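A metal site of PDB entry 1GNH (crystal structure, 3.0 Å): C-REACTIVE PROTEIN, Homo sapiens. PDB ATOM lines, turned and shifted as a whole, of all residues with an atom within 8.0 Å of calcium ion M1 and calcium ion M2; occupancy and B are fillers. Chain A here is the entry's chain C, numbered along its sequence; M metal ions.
OD2 of Asp 60 touches calcium ion M2, 3.3 Å away.
Of the 21 residues printed, 5 come within 4 Å of calcium ion M2.
The nearest printed residue that does not touch calcium ion M2 is Leu 64 (5.2 Å).
Within 4 Å of calcium ion M1: Glu 138, Asp 140, Glu 147 and Gln 150.
The nearest printed residue that does not touch calcium ion M1 is Gln 139 (4.8 Å).
The side-chain carboxylate of Asp 60 lies close to the side-chain amide oxygen of Gln 59 (3.1 Å).
O of Gln 150 sits at hydrogen-bond distance from N of Ser 50.
The backbone NH (N) of Asn 61 sits at hydrogen-bond distance from the side-chain amide oxygen (OE1) of Gln 59 (3.0 Å).
O of Ser 53 sits close to OE1 of Gln 139, 3.3 Å away.
Calcium ion M1 is bound by OE1 of Glu 147, at 2.0 Å.
The side-chain carboxylate (OD2) of Asp 140 binds calcium ion M1 (2.0 Å).
Calcium ion M1 is bound by OE1 of Glu 138 (2.0 Å).
OE1 of Gln 150 is bound to calcium ion M1 (2.3 Å).
Calcium ion M1 is bound by OD1 of Asp 140.
Calcium ion M2 is bound by the side-chain carboxylate (OD1) of Asp 140 (2.0 Å), the backbone carbonyl oxygen (O) of Gln 139 (2.3 Å), the side-chain carboxylate (OE1) of Glu 138 (2.4 Å), the side-chain carboxylate (OE2) of Glu 138 (2.5 Å) and the side-chain amide oxygen (OD1) of Asn 61 (2.7 Å).
Calcium ion M2 has five donor atoms within binding distance.
Slightly farther from calcium ion M2 lies ND2 of Asn 61 (3.1 Å).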
ATOM      1  N   SER A  50     -24.810  26.682 -13.465  1.00  0.00           N
ATOM      2  CA  SER A  50     -25.075  25.267 -13.631  1.00  0.00           C
ATOM      3  C   SER A  50     -25.598  24.962 -15.011  1.00  0.00           C
ATOM      4  O   SER A  50     -26.543  25.582 -15.488  1.00  0.00           O
ATOM      5  CB  SER A  50     -26.086  24.804 -12.595  1.00  0.00           C
ATOM      6  OG  SER A  50     -26.425  23.436 -12.787  1.00  0.00           O
ATOM      7  N   SER A  53     -27.788  19.447 -13.993  1.00  0.00           N
ATOM      8  CA  SER A  53     -27.848  18.993 -12.598  1.00  0.00           C
ATOM      9  C   SER A  53     -28.697  17.724 -12.390  1.00  0.00           C
ATOM     10  O   SER A  53     -29.927  17.775 -12.433  1.00  0.00           O
ATOM     11  CB  SER A  53     -28.383  20.106 -11.707  1.00  0.00           C
ATOM     12  OG  SER A  53     -28.222  19.801 -10.325  1.00  0.00           O
ATOM     13  N   ALA A  55     -29.684  15.066  -9.730  1.00  0.00           N
ATOM     14  CA  ALA A  55     -29.692  14.833  -8.279  1.00  0.00           C
ATOM     15  C   ALA A  55     -30.506  13.636  -7.790  1.00  0.00           C
ATOM     16  O   ALA A  55     -31.533  13.283  -8.366  1.00  0.00           O
ATOM     17  CB  ALA A  55     -30.167  16.087  -7.587  1.00  0.00           C
ATOM     18  N   GLN A  59     -27.821  11.872  -2.738  1.00  0.00           N
ATOM     19  CA  GLN A  59     -26.734  12.744  -3.208  1.00  0.00           C
ATOM     20  C   GLN A  59     -27.303  13.820  -4.137  1.00  0.00           C
ATOM     21  O   GLN A  59     -27.774  13.500  -5.225  1.00  0.00           O
ATOM     22  CB  GLN A  59     -25.674  11.875  -3.923  1.00  0.00           C
ATOM     23  CG  GLN A  59     -24.591  12.629  -4.650  1.00  0.00           C
ATOM     24  CD  GLN A  59     -23.792  13.559  -3.753  1.00  0.00           C
ATOM     25  OE1 GLN A  59     -24.191  14.694  -3.517  1.00  0.00           O
ATOM     26  NE2 GLN A  59     -22.660  13.077  -3.281  1.00  0.00           N
ATOM     27  N   ASP A  60     -27.246  15.071  -3.721  1.00  0.00           N
ATOM     28  CA  ASP A  60     -27.768  16.175  -4.508  1.00  0.00           C
ATOM     29  C   ASP A  60     -26.964  16.464  -5.777  1.00  0.00           C
ATOM     30  O   ASP A  60     -27.480  17.004  -6.767  1.00  0.00           O
ATOM     31  CB  ASP A  60     -27.880  17.458  -3.668  1.00  0.00           C
ATOM     32  CG  ASP A  60     -26.536  17.937  -3.138  1.00  0.00           C
ATOM     33  OD1 ASP A  60     -25.810  17.124  -2.508  1.00  0.00           O
ATOM     34  OD2 ASP A  60     -26.203  19.121  -3.315  1.00  0.00           O
ATOM     35  N   ASN A  61     -25.679  16.116  -5.765  1.00  0.00           N
ATOM     36  CA  ASN A  61     -24.850  16.345  -6.935  1.00  0.00           C
ATOM     37  C   ASN A  61     -24.344  15.021  -7.467  1.00  0.00           C
ATOM     38  O   ASN A  61     -23.139  14.758  -7.456  1.00  0.00           O
ATOM     39  CB  ASN A  61     -23.670  17.263  -6.586  1.00  0.00           C
ATOM     40  CG  ASN A  61     -24.109  18.675  -6.246  1.00  0.00           C
ATOM     41  OD1 ASN A  61     -25.159  19.108  -6.693  1.00  0.00           O
ATOM     42  ND2 ASN A  61     -23.305  19.390  -5.457  1.00  0.00           N
ATOM     43  N   GLU A  62     -25.265  14.167  -7.924  1.00  0.00           N
ATOM     44  CA  GLU A  62     -24.938  12.842  -8.444  1.00  0.00           C
ATOM     45  C   GLU A  62     -24.076  12.968  -9.706  1.00  0.00           C
ATOM     46  O   GLU A  62     -23.123  12.231  -9.900  1.00  0.00           O
ATOM     47  CB  GLU A  62     -26.200  12.037  -8.716  1.00  0.00           C
ATOM     48  CG  GLU A  62     -25.968  10.543  -8.914  1.00  0.00           C
ATOM     49  CD  GLU A  62     -25.467   9.842  -7.657  1.00  0.00           C
ATOM     50  OE1 GLU A  62     -24.421  10.269  -7.108  1.00  0.00           O
ATOM     51  OE2 GLU A  62     -26.110   8.852  -7.223  1.00  0.00           O
ATOM     52  N   LEU A  64     -23.087  16.438 -12.185  1.00  0.00           N
ATOM     53  CA  LEU A  64     -23.290  17.853 -12.411  1.00  0.00           C
ATOM     54  C   LEU A  64     -22.200  18.486 -13.294  1.00  0.00           C
ATOM     55  O   LEU A  64     -21.002  18.258 -13.082  1.00  0.00           O
ATOM     56  CB  LEU A  64     -23.352  18.574 -11.072  1.00  0.00           C
ATOM     57  CG  LEU A  64     -23.279  20.106 -11.047  1.00  0.00           C
ATOM     58  CD1 LEU A  64     -24.577  20.701 -10.574  1.00  0.00           C
ATOM     59  CD2 LEU A  64     -22.174  20.511 -10.134  1.00  0.00           C
ATOM     60  N   PHE A  66     -20.788  22.063 -14.558  1.00  0.00           N
ATOM     61  CA  PHE A  66     -20.814  23.447 -14.120  1.00  0.00           C
ATOM     62  C   PHE A  66     -19.649  24.241 -14.704  1.00  0.00           C
ATOM     63  O   PHE A  66     -18.576  23.681 -14.959  1.00  0.00           O
ATOM     64  CB  PHE A  66     -20.692  23.407 -12.591  1.00  0.00           C
ATOM     65  CG  PHE A  66     -20.943  24.713 -11.916  1.00  0.00           C
ATOM     66  CD1 PHE A  66     -19.907  25.624 -11.684  1.00  0.00           C
ATOM     67  CD2 PHE A  66     -22.215  25.013 -11.448  1.00  0.00           C
ATOM     68  CE1 PHE A  66     -20.139  26.812 -10.992  1.00  0.00           C
ATOM     69  CE2 PHE A  66     -22.459  26.203 -10.765  1.00  0.00           C
ATOM     70  CZ  PHE A  66     -21.422  27.114 -10.533  1.00  0.00           C
ATOM     71  N   GLN A 137     -30.927  25.514 -13.267  1.00  0.00           N
ATOM     72  CA  GLN A 137     -30.780  25.813 -11.851  1.00  0.00           C
ATOM     73  C   GLN A 137     -29.842  24.826 -11.218  1.00  0.00           C
ATOM     74  O   GLN A 137     -29.651  23.716 -11.752  1.00  0.00           O
ATOM     75  CB  GLN A 137     -32.118  25.754 -11.126  1.00  0.00           C
ATOM     76  CG  GLN A 137     -32.948  27.007 -11.278  1.00  0.00           C
ATOM     77  CD  GLN A 137     -32.202  28.279 -10.872  1.00  0.00           C
ATOM     78  OE1 GLN A 137     -32.602  29.390 -11.280  1.00  0.00           O
ATOM     79  NE2 GLN A 137     -31.134  28.143 -10.056  1.00  0.00           N
ATOM     80  N   GLU A 138     -29.261  25.212 -10.077  1.00  0.00           N
ATOM     81  CA  GLU A 138     -28.325  24.335  -9.380  1.00  0.00           C
ATOM     82  C   GLU A 138     -29.005  23.654  -8.200  1.00  0.00           C
ATOM     83  O   GLU A 138     -29.347  24.322  -7.215  1.00  0.00           O
ATOM     84  CB  GLU A 138     -27.106  25.123  -8.902  1.00  0.00           C
ATOM     85  CG  GLU A 138     -25.855  24.279  -8.728  1.00  0.00           C
ATOM     86  CD  GLU A 138     -25.911  23.299  -7.554  1.00  0.00           C
ATOM     87  OE1 GLU A 138     -25.556  23.704  -6.418  1.00  0.00           O
ATOM     88  OE2 GLU A 138     -26.252  22.114  -7.787  1.00  0.00           O
ATOM     89  N   GLN A 139     -29.210  22.343  -8.302  1.00  0.00           N
ATOM     90  CA  GLN A 139     -29.852  21.587  -7.229  1.00  0.00           C
ATOM     91  C   GLN A 139     -28.936  21.345  -6.019  1.00  0.00           C
ATOM     92  O   GLN A 139     -27.763  20.957  -6.135  1.00  0.00           O
ATOM     93  CB  GLN A 139     -30.339  20.242  -7.739  1.00  0.00           C
ATOM     94  CG  GLN A 139     -31.770  20.227  -8.147  1.00  0.00           C
ATOM     95  CD  GLN A 139     -32.077  19.051  -9.067  1.00  0.00           C
ATOM     96  OE1 GLN A 139     -31.968  19.171 -10.279  1.00  0.00           O
ATOM     97  NE2 GLN A 139     -32.410  17.913  -8.487  1.00  0.00           N
ATOM     98  N   ASP A 140     -29.513  21.569  -4.835  1.00  0.00           N
ATOM     99  CA  ASP A 140     -28.809  21.373  -3.586  1.00  0.00           C
ATOM    100  C   ASP A 140     -29.689  20.520  -2.671  1.00  0.00           C
ATOM    101  O   ASP A 140     -29.409  20.341  -1.485  1.00  0.00           O
ATOM    102  CB  ASP A 140     -28.444  22.730  -2.974  1.00  0.00           C
ATOM    103  CG  ASP A 140     -27.294  23.398  -3.719  1.00  0.00           C
ATOM    104  OD1 ASP A 140     -26.349  22.682  -4.121  1.00  0.00           O
ATOM    105  OD2 ASP A 140     -27.335  24.639  -3.913  1.00  0.00           O
ATOM    106  N   SER A 141     -30.759  19.996  -3.261  1.00  0.00           N
ATOM    107  CA  SER A 141     -31.704  19.129  -2.590  1.00  0.00           C
ATOM    108  C   SER A 141     -32.534  18.531  -3.703  1.00  0.00           C
ATOM    109  O   SER A 141     -32.696  19.153  -4.748  1.00  0.00           O
ATOM    110  CB  SER A 141     -32.602  19.905  -1.610  1.00  0.00           C
ATOM    111  OG  SER A 141     -33.682  20.559  -2.244  1.00  0.00           O
ATOM    112  N   GLY A 144     -34.857  20.861  -5.549  1.00  0.00           N
ATOM    113  CA  GLY A 144     -34.946  22.207  -5.022  1.00  0.00           C
ATOM    114  C   GLY A 144     -33.669  22.799  -4.448  1.00  0.00           C
ATOM    115  O   GLY A 144     -32.578  22.299  -4.696  1.00  0.00           O
ATOM    116  N   ASN A 145     -33.844  23.856  -3.651  1.00  0.00           N
ATOM    117  CA  ASN A 145     -32.758  24.582  -2.995  1.00  0.00           C
ATOM    118  C   ASN A 145     -31.880  25.237  -4.041  1.00  0.00           C
ATOM    119  O   ASN A 145     -30.672  25.012  -4.098  1.00  0.00           O
ATOM    120  CB  ASN A 145     -31.946  23.658  -2.084  1.00  0.00           C
ATOM    121  CG  ASN A 145     -32.605  23.458  -0.711  1.00  0.00           C
ATOM    122  OD1 ASN A 145     -33.711  22.915  -0.602  1.00  0.00           O
ATOM    123  ND2 ASN A 145     -31.911  23.877   0.333  1.00  0.00           N
ATOM    124  N   PHE A 146     -32.495  26.102  -4.833  1.00  0.00           N
ATOM    125  CA  PHE A 146     -31.822  26.794  -5.921  1.00  0.00           C
ATOM    126  C   PHE A 146     -31.117  28.074  -5.530  1.00  0.00           C
ATOM    127  O   PHE A 146     -31.735  28.978  -4.970  1.00  0.00           O
ATOM    128  CB  PHE A 146     -32.823  27.100  -7.035  1.00  0.00           C
ATOM    129  CG  PHE A 146     -33.565  25.887  -7.554  1.00  0.00           C
ATOM    130  CD1 PHE A 146     -32.924  24.658  -7.724  1.00  0.00           C
ATOM    131  CD2 PHE A 146     -34.922  25.969  -7.858  1.00  0.00           C
ATOM    132  CE1 PHE A 146     -33.626  23.553  -8.186  1.00  0.00           C
ATOM    133  CE2 PHE A 146     -35.618  24.852  -8.319  1.00  0.00           C
ATOM    134  CZ  PHE A 146     -34.966  23.655  -8.475  1.00  0.00           C
ATOM    135  N   GLU A 147     -29.834  28.166  -5.830  1.00  0.00           N
ATOM    136  CA  GLU A 147     -29.078  29.385  -5.560  1.00  0.00           C
ATOM    137  C   GLU A 147     -29.061  30.180  -6.851  1.00  0.00           C
ATOM    138  O   GLU A 147     -28.561  29.704  -7.875  1.00  0.00           O
ATOM    139  CB  GLU A 147     -27.655  29.055  -5.144  1.00  0.00           C
ATOM    140  CG  GLU A 147     -27.584  28.369  -3.825  1.00  0.00           C
ATOM    141  CD  GLU A 147     -26.192  27.933  -3.498  1.00  0.00           C
ATOM    142  OE1 GLU A 147     -25.736  26.955  -4.161  1.00  0.00           O
ATOM    143  OE2 GLU A 147     -25.581  28.555  -2.598  1.00  0.00           O
ATOM    144  N   GLY A 148     -29.620  31.381  -6.804  1.00  0.00           N
ATOM    145  CA  GLY A 148     -29.674  32.241  -7.981  1.00  0.00           C
ATOM    146  C   GLY A 148     -28.334  32.664  -8.542  1.00  0.00           C
ATOM    147  O   GLY A 148     -28.253  33.123  -9.694  1.00  0.00           O
ATOM    148  N   SER A 149     -27.285  32.508  -7.750  1.00  0.00           N
ATOM    149  CA  SER A 149     -25.927  32.855  -8.147  1.00  0.00           C
ATOM    150  C   SER A 149     -25.343  31.769  -9.051  1.00  0.00           C
ATOM    151  O   SER A 149     -24.214  31.875  -9.532  1.00  0.00           O
ATOM    152  CB  SER A 149     -25.063  33.011  -6.882  1.00  0.00           C
ATOM    153  OG  SER A 149     -23.763  33.504  -7.171  1.00  0.00           O
ATOM    154  N   GLN A 150     -26.127  30.717  -9.272  1.00  0.00           N
ATOM    155  CA  GLN A 150     -25.698  29.606 -10.093  1.00  0.00           C
ATOM    156  C   GLN A 150     -26.746  29.272 -11.142  1.00  0.00           C
ATOM    157  O   GLN A 150     -26.785  28.163 -11.666  1.00  0.00           O
ATOM    158  CB  GLN A 150     -25.425  28.400  -9.205  1.00  0.00           C
ATOM    159  CG  GLN A 150     -24.584  28.744  -7.979  1.00  0.00           C
ATOM    160  CD  GLN A 150     -24.104  27.508  -7.214  1.00  0.00           C
ATOM    161  OE1 GLN A 150     -24.897  26.678  -6.770  1.00  0.00           O
ATOM    162  NE2 GLN A 150     -22.788  27.409  -7.044  1.00  0.00           N
HETATM  163 CA    CA M   1     -26.004  25.309  -5.245  1.00  0.00          CA
HETATM  164 CA    CA M   2     -25.569  21.501  -5.506  1.00  0.00          CA
